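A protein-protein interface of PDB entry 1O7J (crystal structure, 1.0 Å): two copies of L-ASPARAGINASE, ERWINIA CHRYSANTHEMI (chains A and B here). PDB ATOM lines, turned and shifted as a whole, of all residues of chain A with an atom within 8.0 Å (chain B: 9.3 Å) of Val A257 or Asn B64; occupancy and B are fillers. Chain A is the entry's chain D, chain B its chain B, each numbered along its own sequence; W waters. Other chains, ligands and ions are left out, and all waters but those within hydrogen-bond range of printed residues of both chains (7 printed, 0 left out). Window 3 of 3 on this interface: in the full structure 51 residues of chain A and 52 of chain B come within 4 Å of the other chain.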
ATOM      1  N   TYR A 226     -29.976 -16.176 -26.363  1.00  0.00           N
ATOM      2  CA  TYR A 226     -31.296 -16.171 -25.716  1.00  0.00           C
ATOM      3  C   TYR A 226     -31.141 -16.873 -24.368  1.00  0.00           C
ATOM      4  O   TYR A 226     -30.153 -17.567 -24.111  1.00  0.00           O
ATOM      5  CB  TYR A 226     -32.347 -16.864 -26.591  1.00  0.00           C
ATOM      6  CG  TYR A 226     -32.018 -18.260 -27.069  1.00  0.00           C
ATOM      7  CD1 TYR A 226     -31.159 -18.479 -28.154  1.00  0.00           C
ATOM      8  CD2 TYR A 226     -32.586 -19.380 -26.450  1.00  0.00           C
ATOM      9  CE1 TYR A 226     -30.855 -19.766 -28.588  1.00  0.00           C
ATOM     10  CE2 TYR A 226     -32.318 -20.653 -26.932  1.00  0.00           C
ATOM     11  CZ  TYR A 226     -31.462 -20.850 -27.981  1.00  0.00           C
ATOM     12  OH  TYR A 226     -31.214 -22.105 -28.517  1.00  0.00           O
ATOM     13  N   GLN A 227     -32.140 -16.698 -23.503  1.00  0.00           N
ATOM     14  CA  GLN A 227     -32.138 -17.395 -22.233  1.00  0.00           C
ATOM     15  C   GLN A 227     -32.033 -18.905 -22.480  1.00  0.00           C
ATOM     16  O   GLN A 227     -32.737 -19.449 -23.335  1.00  0.00           O
ATOM     17  CB  GLN A 227     -33.409 -17.112 -21.422  1.00  0.00           C
ATOM     18  CG  GLN A 227     -33.533 -15.678 -20.933  1.00  0.00           C
ATOM     19  CD  GLN A 227     -34.762 -15.454 -20.101  1.00  0.00           C
ATOM     20  OE1 GLN A 227     -35.627 -16.315 -19.965  1.00  0.00           O
ATOM     21  NE2 GLN A 227     -34.833 -14.287 -19.485  1.00  0.00           N
ATOM     22  N   ASP A 228     -31.175 -19.578 -21.688  1.00  0.00           N
ATOM     23  CA  ASP A 228     -30.995 -21.046 -21.782  1.00  0.00           C
ATOM     24  C   ASP A 228     -30.323 -21.494 -23.058  1.00  0.00           C
ATOM     25  O   ASP A 228     -30.360 -22.670 -23.415  1.00  0.00           O
ATOM     26  CB  ASP A 228     -32.291 -21.833 -21.560  1.00  0.00           C
ATOM     27  CG  ASP A 228     -32.974 -21.496 -20.267  1.00  0.00           C
ATOM     28  OD1 ASP A 228     -32.356 -21.751 -19.201  1.00  0.00           O
ATOM     29  OD2 ASP A 228     -34.130 -20.977 -20.301  1.00  0.00           O
ATOM     30  N   ASP A 229     -29.628 -20.586 -23.793  1.00  0.00           N
ATOM     31  CA  ASP A 229     -28.956 -20.989 -24.985  1.00  0.00           C
ATOM     32  C   ASP A 229     -27.952 -22.119 -24.744  1.00  0.00           C
ATOM     33  O   ASP A 229     -27.223 -22.119 -23.758  1.00  0.00           O
ATOM     34  CB  ASP A 229     -28.271 -19.807 -25.677  1.00  0.00           C
ATOM     35  CG  ASP A 229     -27.247 -19.053 -24.874  1.00  0.00           C
ATOM     36  OD1 ASP A 229     -27.185 -19.078 -23.635  1.00  0.00           O
ATOM     37  OD2 ASP A 229     -26.491 -18.359 -25.564  1.00  0.00           O
ATOM     38  N   GLU A 231     -24.768 -24.858 -24.982  1.00  0.00           N
ATOM     39  CA  GLU A 231     -23.399 -25.049 -25.398  1.00  0.00           C
ATOM     40  C   GLU A 231     -23.290 -25.997 -26.593  1.00  0.00           C
ATOM     41  O   GLU A 231     -22.370 -25.828 -27.425  1.00  0.00           O
ATOM     42  CB  GLU A 231     -22.618 -25.609 -24.196  1.00  0.00           C
ATOM     43  CG  GLU A 231     -21.108 -25.529 -24.346  1.00  0.00           C
ATOM     44  CD  GLU A 231     -20.449 -25.942 -23.027  1.00  0.00           C
ATOM     45  OE1 GLU A 231     -21.191 -26.032 -22.003  1.00  0.00           O
ATOM     46  OE2 GLU A 231     -19.220 -26.189 -22.979  1.00  0.00           O
ATOM     47  N   MET A 250     -27.472 -11.562 -27.330  1.00  0.00           N
ATOM     48  CA  MET A 250     -28.349 -10.786 -26.449  1.00  0.00           C
ATOM     49  C   MET A 250     -27.778  -9.388 -26.325  1.00  0.00           C
ATOM     50  O   MET A 250     -26.589  -9.238 -26.069  1.00  0.00           O
ATOM     51  CB  MET A 250     -28.456 -11.525 -25.096  1.00  0.00           C
ATOM     52  CG  MET A 250     -29.176 -12.854 -25.193  1.00  0.00           C
ATOM     53  SD  MET A 250     -29.156 -13.858 -23.723  1.00  0.00           S
ATOM     54  CE  MET A 250     -27.587 -14.700 -23.915  1.00  0.00           C
ATOM     55  N   SER A 254     -23.779  -9.718 -25.589  1.00  0.00           N
ATOM     56  CA  SER A 254     -23.559 -10.323 -24.280  1.00  0.00           C
ATOM     57  C   SER A 254     -23.723 -11.832 -24.358  1.00  0.00           C
ATOM     58  O   SER A 254     -24.534 -12.296 -25.189  1.00  0.00           O
ATOM     59  CB  SER A 254     -24.485  -9.719 -23.227  1.00  0.00           C
ATOM     60  OG  SER A 254     -24.276  -8.308 -23.087  1.00  0.00           O
ATOM     61  N   VAL A 255     -23.002 -12.552 -23.510  1.00  0.00           N
ATOM     62  CA  VAL A 255     -22.861 -13.991 -23.617  1.00  0.00           C
ATOM     63  C   VAL A 255     -23.138 -14.656 -22.275  1.00  0.00           C
ATOM     64  O   VAL A 255     -22.577 -14.261 -21.235  1.00  0.00           O
ATOM     65  CB  VAL A 255     -21.414 -14.362 -24.123  1.00  0.00           C
ATOM     66  CG1 VAL A 255     -21.450 -15.806 -24.574  1.00  0.00           C
ATOM     67  CG2 VAL A 255     -20.900 -13.451 -25.223  1.00  0.00           C
ATOM     68  N   SER A 256     -23.985 -15.684 -22.274  1.00  0.00           N
ATOM     69  CA  SER A 256     -24.262 -16.448 -21.063  1.00  0.00           C
ATOM     70  C   SER A 256     -23.050 -17.312 -20.697  1.00  0.00           C
ATOM     71  O   SER A 256     -22.142 -17.514 -21.497  1.00  0.00           O
ATOM     72  CB  SER A 256     -25.455 -17.371 -21.274  1.00  0.00           C
ATOM     73  OG  SER A 256     -25.066 -18.460 -22.135  1.00  0.00           O
ATOM     74  N   VAL A 257     -23.090 -17.928 -19.490  1.00  0.00           N
ATOM     75  CA  VAL A 257     -22.031 -18.820 -19.071  1.00  0.00           C
ATOM     76  C   VAL A 257     -21.859 -19.955 -20.107  1.00  0.00           C
ATOM     77  O   VAL A 257     -20.726 -20.387 -20.385  1.00  0.00           O
ATOM     78  CB  VAL A 257     -22.370 -19.376 -17.671  1.00  0.00           C
ATOM     79  CG1 VAL A 257     -23.765 -19.984 -17.707  1.00  0.00           C
ATOM     80  CG2 VAL A 257     -21.383 -20.405 -17.166  1.00  0.00           C
ATOM     81  N   ARG A 258     -22.941 -20.452 -20.672  1.00  0.00           N
ATOM     82  CA  ARG A 258     -22.914 -21.515 -21.637  1.00  0.00           C
ATOM     83  C   ARG A 258     -22.323 -21.048 -22.973  1.00  0.00           C
ATOM     84  O   ARG A 258     -21.514 -21.754 -23.596  1.00  0.00           O
ATOM     85  CB  ARG A 258     -24.322 -22.090 -21.831  1.00  0.00           C
ATOM     86  CG  ARG A 258     -24.891 -22.739 -20.588  1.00  0.00           C
ATOM     87  CD  ARG A 258     -26.397 -23.060 -20.652  1.00  0.00           C
ATOM     88  NE  ARG A 258     -27.128 -21.884 -21.075  1.00  0.00           N
ATOM     89  CZ  ARG A 258     -27.405 -20.849 -20.284  1.00  0.00           C
ATOM     90  NH1 ARG A 258     -27.177 -20.902 -18.996  1.00  0.00           N
ATOM     91  NH2 ARG A 258     -27.943 -19.785 -20.841  1.00  0.00           N
ATOM     92  N   GLY A 259     -22.723 -19.860 -23.439  1.00  0.00           N
ATOM     93  CA  GLY A 259     -22.135 -19.311 -24.637  1.00  0.00           C
ATOM     94  C   GLY A 259     -20.639 -19.079 -24.510  1.00  0.00           C
ATOM     95  O   GLY A 259     -19.882 -19.286 -25.447  1.00  0.00           O
ATOM     96  N   ILE A 260     -20.209 -18.645 -23.320  1.00  0.00           N
ATOM     97  CA  ILE A 260     -18.779 -18.406 -23.107  1.00  0.00           C
ATOM     98  C   ILE A 260     -18.028 -19.705 -23.215  1.00  0.00           C
ATOM     99  O   ILE A 260     -16.949 -19.761 -23.856  1.00  0.00           O
ATOM    100  CB  ILE A 260     -18.543 -17.666 -21.763  1.00  0.00           C
ATOM    101  CG1 ILE A 260     -19.080 -16.242 -21.822  1.00  0.00           C
ATOM    102  CG2 ILE A 260     -17.053 -17.724 -21.408  1.00  0.00           C
ATOM    103  CD1 ILE A 260     -19.089 -15.480 -20.531  1.00  0.00           C
ATOM    104  N   ALA A 261     -18.532 -20.772 -22.593  1.00  0.00           N
ATOM    105  CA  ALA A 261     -17.872 -22.078 -22.680  1.00  0.00           C
ATOM    106  C   ALA A 261     -17.794 -22.526 -24.137  1.00  0.00           C
ATOM    107  O   ALA A 261     -16.751 -23.020 -24.619  1.00  0.00           O
ATOM    108  CB  ALA A 261     -18.606 -23.105 -21.823  1.00  0.00           C
ATOM    109  N   GLY A 262     -18.892 -22.346 -24.901  1.00  0.00           N
ATOM    110  CA  GLY A 262     -18.886 -22.728 -26.299  1.00  0.00           C
ATOM    111  C   GLY A 262     -17.891 -21.933 -27.129  1.00  0.00           C
ATOM    112  O   GLY A 262     -17.171 -22.480 -28.005  1.00  0.00           O
ATOM    113  N   MET A 263     -17.856 -20.631 -26.904  1.00  0.00           N
ATOM    114  CA  MET A 263     -16.925 -19.760 -27.645  1.00  0.00           C
ATOM    115  C   MET A 263     -15.483 -20.067 -27.288  1.00  0.00           C
ATOM    116  O   MET A 263     -14.628 -20.049 -28.203  1.00  0.00           O
ATOM    117  CB  MET A 263     -17.201 -18.295 -27.316  1.00  0.00           C
ATOM    118  CG  MET A 263     -18.495 -17.775 -27.923  1.00  0.00           C
ATOM    119  SD  MET A 263     -18.788 -16.083 -27.472  1.00  0.00           S
ATOM    120  CE  MET A 263     -20.374 -15.822 -28.306  1.00  0.00           C
ATOM    121  N   ARG A 264     -15.193 -20.370 -26.040  1.00  0.00           N
ATOM    122  CA  ARG A 264     -13.802 -20.720 -25.693  1.00  0.00           C
ATOM    123  C   ARG A 264     -13.416 -22.037 -26.371  1.00  0.00           C
ATOM    124  O   ARG A 264     -12.275 -22.174 -26.863  1.00  0.00           O
ATOM    125  CB  ARG A 264     -13.648 -20.761 -24.171  1.00  0.00           C
ATOM    126  CG  ARG A 264     -13.688 -19.388 -23.507  1.00  0.00           C
ATOM    127  N   THR B  12     -33.714  -8.521  -9.325  1.00  0.00           N
ATOM    128  CA  THR B  12     -33.090  -9.700  -9.928  1.00  0.00           C
ATOM    129  C   THR B  12     -31.687  -9.462 -10.406  1.00  0.00           C
ATOM    130  O   THR B  12     -31.007 -10.461 -10.791  1.00  0.00           O
ATOM    131  CB  THR B  12     -33.920 -10.239 -11.129  1.00  0.00           C
ATOM    132  OG1 THR B  12     -33.784  -9.390 -12.272  1.00  0.00           O
ATOM    133  CG2 THR B  12     -35.394 -10.409 -10.781  1.00  0.00           C
ATOM    134  N   GLY B  14     -29.136  -7.002 -13.120  1.00  0.00           N
ATOM    135  CA  GLY B  14     -29.087  -6.140 -14.273  1.00  0.00           C
ATOM    136  C   GLY B  14     -28.147  -4.962 -14.119  1.00  0.00           C
ATOM    137  O   GLY B  14     -27.654  -4.604 -13.064  1.00  0.00           O
ATOM    138  N   ALA B  31     -22.853  -6.002 -14.198  1.00  0.00           N
ATOM    139  CA  ALA B  31     -24.316  -6.052 -14.033  1.00  0.00           C
ATOM    140  C   ALA B  31     -24.641  -6.897 -12.795  1.00  0.00           C
ATOM    141  O   ALA B  31     -24.075  -7.992 -12.526  1.00  0.00           O
ATOM    142  CB  ALA B  31     -24.985  -6.501 -15.354  1.00  0.00           C
ATOM    143  N   SER B  58     -32.640 -12.226  -6.769  1.00  0.00           N
ATOM    144  CA  SER B  58     -31.388 -12.686  -7.354  1.00  0.00           C
ATOM    145  C   SER B  58     -30.520 -11.483  -7.629  1.00  0.00           C
ATOM    146  O   SER B  58     -30.926 -10.350  -7.415  1.00  0.00           O
ATOM    147  CB  SER B  58     -31.599 -13.511  -8.652  1.00  0.00           C
ATOM    148  OG  SER B  58     -32.267 -12.763  -9.687  1.00  0.00           O
ATOM    149  N   ASN B  59     -29.286 -11.700  -8.131  1.00  0.00           N
ATOM    150  CA  ASN B  59     -28.444 -10.554  -8.471  1.00  0.00           C
ATOM    151  C   ASN B  59     -27.502 -11.011  -9.593  1.00  0.00           C
ATOM    152  O   ASN B  59     -26.357 -11.365  -9.408  1.00  0.00           O
ATOM    153  CB  ASN B  59     -27.714  -9.923  -7.283  1.00  0.00           C
ATOM    154  CG  ASN B  59     -27.776  -8.355  -7.329  1.00  0.00           C
ATOM    155  OD1 ASN B  59     -28.228  -7.695  -8.273  1.00  0.00           O
ATOM    156  ND2 ASN B  59     -27.312  -7.735  -6.274  1.00  0.00           N
ATOM    157  N   MET B  60     -28.048 -11.060 -10.829  1.00  0.00           N
ATOM    158  CA  MET B  60     -27.326 -11.550 -12.002  1.00  0.00           C
ATOM    159  C   MET B  60     -27.539 -10.622 -13.196  1.00  0.00           C
ATOM    160  O   MET B  60     -28.538  -9.919 -13.303  1.00  0.00           O
ATOM    161  CB  MET B  60     -27.718 -12.977 -12.377  1.00  0.00           C
ATOM    162  CG  MET B  60     -29.101 -13.088 -12.971  1.00  0.00           C
ATOM    163  SD  MET B  60     -29.623 -14.789 -13.352  1.00  0.00           S
ATOM    164  CE  MET B  60     -30.155 -15.292 -11.711  1.00  0.00           C
ATOM    165  N   ALA B  61     -26.588 -10.700 -14.105  1.00  0.00           N
ATOM    166  CA  ALA B  61     -26.726 -10.081 -15.428  1.00  0.00           C
ATOM    167  C   ALA B  61     -27.749 -10.849 -16.224  1.00  0.00           C
ATOM    168  O   ALA B  61     -27.786 -12.097 -16.179  1.00  0.00           O
ATOM    169  CB  ALA B  61     -25.366 -10.042 -16.101  1.00  0.00           C
ATOM    170  N   SER B  62     -28.584 -10.157 -17.024  1.00  0.00           N
ATOM    171  CA  SER B  62     -29.741 -10.874 -17.585  1.00  0.00           C
ATOM    172  C   SER B  62     -29.416 -11.831 -18.710  1.00  0.00           C
ATOM    173  O   SER B  62     -30.278 -12.712 -18.984  1.00  0.00           O
ATOM    174  CB  SER B  62     -30.878  -9.950 -17.982  1.00  0.00           C
ATOM    175  OG  SER B  62     -30.630  -9.213 -19.170  1.00  0.00           O
ATOM    176  N   GLU B  63     -28.238 -11.769 -19.295  1.00  0.00           N
ATOM    177  CA  GLU B  63     -27.855 -12.805 -20.269  1.00  0.00           C
ATOM    178  C   GLU B  63     -27.758 -14.190 -19.556  1.00  0.00           C
ATOM    179  O   GLU B  63     -27.753 -15.218 -20.258  1.00  0.00           O
ATOM    180  CB  GLU B  63     -26.545 -12.485 -20.996  1.00  0.00           C
ATOM    181  CG  GLU B  63     -25.293 -12.457 -20.103  1.00  0.00           C
ATOM    182  CD  GLU B  63     -24.982 -11.127 -19.471  1.00  0.00           C
ATOM    183  OE1 GLU B  63     -25.869 -10.310 -19.249  1.00  0.00           O
ATOM    184  OE2 GLU B  63     -23.784 -10.827 -19.231  1.00  0.00           O
ATOM    185  N   ASN B  64     -27.674 -14.210 -18.240  1.00  0.00           N
ATOM    186  CA  ASN B  64     -27.618 -15.465 -17.463  1.00  0.00           C
ATOM    187  C   ASN B  64     -28.923 -15.872 -16.852  1.00  0.00           C
ATOM    188  O   ASN B  64     -28.985 -16.930 -16.189  1.00  0.00           O
ATOM    189  CB  ASN B  64     -26.519 -15.390 -16.361  1.00  0.00           C
ATOM    190  CG  ASN B  64     -25.177 -15.698 -17.064  1.00  0.00           C
ATOM    191  OD1 ASN B  64     -25.056 -16.746 -17.740  1.00  0.00           O
ATOM    192  ND2 ASN B  64     -24.227 -14.867 -16.758  1.00  0.00           N
ATOM    193  N   MET B  65     -29.998 -15.117 -17.059  1.00  0.00           N
ATOM    194  CA  MET B  65     -31.338 -15.495 -16.570  1.00  0.00           C
ATOM    195  C   MET B  65     -31.762 -16.781 -17.313  1.00  0.00           C
ATOM    196  O   MET B  65     -31.593 -16.877 -18.548  1.00  0.00           O
ATOM    197  CB  MET B  65     -32.313 -14.365 -16.781  1.00  0.00           C
ATOM    198  CG  MET B  65     -33.699 -14.602 -16.221  1.00  0.00           C
ATOM    199  SD  MET B  65     -33.832 -15.027 -14.495  1.00  0.00           S
ATOM    200  CE  MET B  65     -33.134 -13.564 -13.755  1.00  0.00           C
ATOM    201  N   THR B  66     -32.335 -17.721 -16.615  1.00  0.00           N
ATOM    202  CA  THR B  66     -32.730 -19.030 -17.131  1.00  0.00           C
ATOM    203  C   THR B  66     -34.204 -19.280 -16.838  1.00  0.00           C
ATOM    204  O   THR B  66     -34.771 -18.770 -15.846  1.00  0.00           O
ATOM    205  CB  THR B  66     -31.880 -20.127 -16.511  1.00  0.00           C
ATOM    206  OG1 THR B  66     -31.945 -20.046 -15.098  1.00  0.00           O
ATOM    207  CG2 THR B  66     -30.430 -20.022 -16.972  1.00  0.00           C
ATOM    208  N   GLY B  67     -34.816 -20.135 -17.668  1.00  0.00           N
ATOM    209  CA  GLY B  67     -36.224 -20.474 -17.442  1.00  0.00           C
ATOM    210  C   GLY B  67     -36.540 -21.008 -16.075  1.00  0.00           C
ATOM    211  O   GLY B  67     -37.611 -20.715 -15.525  1.00  0.00           O
ATOM    212  N   ASP B  68     -35.673 -21.828 -15.495  1.00  0.00           N
ATOM    213  CA  ASP B  68     -35.939 -22.319 -14.164  1.00  0.00           C
ATOM    214  C   ASP B  68     -36.027 -21.233 -13.133  1.00  0.00           C
ATOM    215  O   ASP B  68     -36.851 -21.321 -12.195  1.00  0.00           O
ATOM    216  CB  ASP B  68     -34.879 -23.386 -13.821  1.00  0.00           C
ATOM    217  CG  ASP B  68     -35.142 -24.707 -14.527  1.00  0.00           C
ATOM    218  OD1 ASP B  68     -35.989 -24.894 -15.415  1.00  0.00           O
ATOM    219  OD2 ASP B  68     -34.428 -25.613 -14.054  1.00  0.00           O
ATOM    220  N   VAL B  69     -35.222 -20.203 -13.286  1.00  0.00           N
ATOM    221  CA  VAL B  69     -35.290 -19.045 -12.389  1.00  0.00           C
ATOM    222  C   VAL B  69     -36.498 -18.201 -12.701  1.00  0.00           C
ATOM    223  O   VAL B  69     -37.176 -17.718 -11.767  1.00  0.00           O
ATOM    224  CB  VAL B  69     -33.961 -18.284 -12.415  1.00  0.00           C
ATOM    225  CG1 VAL B  69     -34.037 -16.961 -11.604  1.00  0.00           C
ATOM    226  CG2 VAL B  69     -32.799 -19.136 -11.913  1.00  0.00           C
ATOM    227  N   VAL B  70     -36.836 -17.992 -13.971  1.00  0.00           N
ATOM    228  CA  VAL B  70     -38.034 -17.248 -14.347  1.00  0.00           C
ATOM    229  C   VAL B  70     -39.289 -17.920 -13.763  1.00  0.00           C
ATOM    230  O   VAL B  70     -40.224 -17.238 -13.339  1.00  0.00           O
ATOM    231  CB  VAL B  70     -38.119 -17.004 -15.837  1.00  0.00           C
ATOM    232  CG1 VAL B  70     -39.397 -16.183 -16.236  1.00  0.00           C
ATOM    233  CG2 VAL B  70     -36.922 -16.230 -16.381  1.00  0.00           C
ATOM    234  N   HIS B  93     -34.480  -5.603 -13.418  1.00  0.00           N
ATOM    235  CA  HIS B  93     -33.968  -6.687 -14.248  1.00  0.00           C
ATOM    236  C   HIS B  93     -32.997  -6.113 -15.268  1.00  0.00           C
ATOM    237  O   HIS B  93     -33.025  -4.913 -15.609  1.00  0.00           O
ATOM    238  CB  HIS B  93     -35.157  -7.361 -14.956  1.00  0.00           C
ATOM    239  CG  HIS B  93     -34.996  -8.690 -15.636  1.00  0.00           C
ATOM    240  ND1 HIS B  93     -34.395  -8.835 -16.894  1.00  0.00           N
ATOM    241  CD2 HIS B  93     -35.419  -9.926 -15.316  1.00  0.00           C
ATOM    242  CE1 HIS B  93     -34.474 -10.128 -17.214  1.00  0.00           C
ATOM    243  NE2 HIS B  93     -35.089 -10.846 -16.290  1.00  0.00           N
ATOM    244  N   GLY B  94     -32.156  -6.981 -15.822  1.00  0.00           N
ATOM    245  CA  GLY B  94     -31.312  -6.571 -16.924  1.00  0.00           C
ATOM    246  C   GLY B  94     -32.070  -6.313 -18.216  1.00  0.00           C
ATOM    247  O   GLY B  94     -33.180  -6.834 -18.433  1.00  0.00           O
ATOM    248  N   ASP B  96     -30.982  -7.066 -21.432  1.00  0.00           N
ATOM    249  CA  ASP B  96     -30.750  -7.979 -22.555  1.00  0.00           C
ATOM    250  C   ASP B  96     -31.885  -8.987 -22.742  1.00  0.00           C
ATOM    251  O   ASP B  96     -32.235  -9.273 -23.876  1.00  0.00           O
ATOM    252  CB  ASP B  96     -29.448  -8.748 -22.347  1.00  0.00           C
ATOM    253  CG  ASP B  96     -28.195  -7.937 -22.524  1.00  0.00           C
ATOM    254  OD1 ASP B  96     -28.283  -6.759 -22.938  1.00  0.00           O
ATOM    255  OD2 ASP B  96     -27.123  -8.531 -22.274  1.00  0.00           O
ATOM    256  N   THR B  97     -32.424  -9.530 -21.644  1.00  0.00           N
ATOM    257  CA  THR B  97     -33.467 -10.558 -21.746  1.00  0.00           C
ATOM    258  C   THR B  97     -34.750 -10.156 -20.998  1.00  0.00           C
ATOM    259  O   THR B  97     -35.596 -11.036 -20.743  1.00  0.00           O
ATOM    260  CB  THR B  97     -33.004 -11.964 -21.309  1.00  0.00           C
ATOM    261  OG1 THR B  97     -32.826 -11.992 -19.897  1.00  0.00           O
ATOM    262  CG2 THR B  97     -31.744 -12.369 -22.055  1.00  0.00           C
ATOM    263  N   GLU B 100     -37.935 -11.460 -22.592  1.00  0.00           N
ATOM    264  CA  GLU B 100     -38.215 -12.895 -22.349  1.00  0.00           C
ATOM    265  C   GLU B 100     -38.857 -13.095 -20.973  1.00  0.00           C
ATOM    266  O   GLU B 100     -39.934 -13.715 -20.864  1.00  0.00           O
ATOM    267  CB  GLU B 100     -36.918 -13.674 -22.506  1.00  0.00           C
ATOM    268  CG  GLU B 100     -36.449 -13.699 -23.997  1.00  0.00           C
ATOM    269  CD  GLU B 100     -35.027 -14.102 -24.183  1.00  0.00           C
ATOM    270  OE1 GLU B 100     -34.737 -15.348 -24.225  1.00  0.00           O
ATOM    271  OE2 GLU B 100     -34.148 -13.208 -24.257  1.00  0.00           O
ATOM    272  N   SER B 101     -38.241 -12.591 -19.908  1.00  0.00           N
ATOM    273  CA  SER B 101     -38.813 -12.736 -18.585  1.00  0.00           C
ATOM    274  C   SER B 101     -40.189 -12.080 -18.483  1.00  0.00           C
ATOM    275  O   SER B 101     -41.119 -12.625 -17.865  1.00  0.00           O
ATOM    276  CB  SER B 101     -37.886 -12.112 -17.507  1.00  0.00           C
ATOM    277  OG  SER B 101     -36.647 -12.793 -17.522  1.00  0.00           O
HETATM  278  O   HOH W   1     -29.296 -17.512 -19.906  1.00  0.00           O
HETATM  279  O   HOH W   2     -21.928 -14.752 -18.556  1.00  0.00           O
HETATM  280  O   HOH W   3     -26.919 -18.763 -16.983  1.00  0.00           O
HETATM  281  O   HOH W   4     -25.761  -5.923 -23.549  1.00  0.00           O
HETATM  282  O   HOH W   5     -21.828 -11.037 -21.309  1.00  0.00           O
HETATM  283  O   HOH W   6     -25.423  -7.772 -20.246  1.00  0.00           O
HETATM  284  O   HOH W   7     -33.717 -23.198 -17.302  1.00  0.00           O
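OD2 of Asp A228 sits at hydrogen-bond distance from N of Gly B67 (2.8 Å).
The side-chain carboxylate (OE1) of Glu B100 is in hydrogen-bond range of the backbone NH (N) of Gln A227, at 3.0 Å.
The backbone NH (N) of Val A257 lies within hydrogen-bond range of the side-chain amide oxygen (OD1) of Asn B64 (2.9 Å).
The side-chain carboxylate (OD2) of Asp B96 sits at hydrogen-bond distance from the side-chain hydroxyl (OG) of Ser A254 (3.0 Å).
OG of Ser B101 is in hydrogen-bond range of NE2 of Gln A227.
The side-chain amide nitrogen (NE2) of Gln A227 is in hydrogen-bond range of the side-chain hydroxyl (OG1) of Thr B97 (3.1 Å).
SD of Met B60 sits close to N of Met B65 (3.7 Å).
The backbone carbonyl oxygen (O) of Ser B62 sits at hydrogen-bond distance from the side-chain hydroxyl (OG1) of Thr B97 (2.8 Å).
N of Asp B96 lies within hydrogen-bond range of OG of Ser B62, 3.1 Å away.
The guanidinium group (NH2) of Arg A258 lies within salt-bridge range of the side-chain carboxylate (OD1) of Asp A229, 3.0 Å away.
The backbone NH of Tyr A226 sits at hydrogen-bond distance from the side-chain sulfur of Met A250, at 3.6 Å.
The side-chain hydroxyl (OG) of Ser A256 sits at hydrogen-bond distance from the backbone NH (N) of Gly A259, at 3.0 Å.
No position is printed for both chains.
Of the 17 pairs that touch across the chains among the printed residues, none has its exchanged pair printed and touching as well.
Water W4 bridges the side-chain carboxylate of Asp B96 and the side-chain hydroxyl of Ser A254.
Water W1 lies within hydrogen-bond range of the backbone carbonyl oxygen of Met B65, the backbone carbonyl oxygen of Glu B63, the guanidinium group of Arg A258 and the backbone NH of Asp A228.
Water W7 lies within hydrogen-bond range of OD1 of Asp A228, N of Asp B68 and N of Gly B67.
Water W6 lies within hydrogen-bond range of the side-chain carboxylate (OD2) of Asp B96 (2.8 Å), the side-chain carboxylate (OE1) of Glu B63 (2.8 Å) and the side-chain hydroxyl (OG) of Ser A254 (3.1 Å).
Water W2 bridges O of Val A255 and ND2 of Asn B64.
Water W3 bridges OD1 of Asn B64 (2.8 Å) and NH1 of Arg A258 (2.9 Å).
Printed residues of chain B within 4 Å of Gln A227: Met B65, Val B70, Thr B97, Glu B100 and Ser B101.
Of the printed residues of chain B, Ser A254 touches Asp B96 (3.0 Å).
Ser A256 touches just these residues of chain B: Glu B63 (3.3 Å) and Asn B64 (3.4 Å).
Of the printed residues of chain B, Val A257 touches Asn B64.
No residue of chain B comes within 4 Å of Gly A259.
No residue of chain B comes within 4 Å of Ile A260.
Of the printed residues of chain A, Glu B63 touches Met A250, Val A255 and Ser A256.
Printed residues of chain A within 4 Å of Asn B64: Ser A256 and Val A257.
Of the printed residues of chain A, Gly B67 touches Asp A228 (2.8 Å).
Printed residues of chain A within 4 Å of Ser B101: Gln A227 (3.1 Å).
The nearest printed residue of chain B that does not touch Val A257 is Glu B63 (5.4 Å).
The nearest printed residue of chain A that does not touch Asn B64 is Val A255 (4.8 Å).
CB of Tyr A226 touches OE1 of Glu B100, at 3.7 Å.
Met B65 touches Gln A227 (O to CG, 3.3 Å).
CG2 of Val B70 touches OE1 of Gln A227, at 3.8 Å.
CB of Thr B66 touches OD1 of Asp A228 (3.2 Å).
O of Glu B63 touches CE of Met A250 (3.7 Å).
Met A250 touches Asp B96 (O to OD2, 3.9 Å).
SD of Met A250 touches CG2 of Thr B97, at 3.4 Å.
Val A255 touches Glu B63 (O to CG, 3.5 Å).
Asn B64 touches Ser A256.
Thr B66 touches Arg A258 (CG2 to NH1, 3.9 Å).
Of the 22 printed residues of chain B, 10 touch a printed residue of chain A.
Hydrophobic or aromatic side chains of chain B within 4 Å of the printed part of chain A: Met B65 and Val B70.
Of the 17 printed residues of chain A, 9 touch a printed residue of chain B.
Among the printed residues, 17 pairs touch across the chains.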
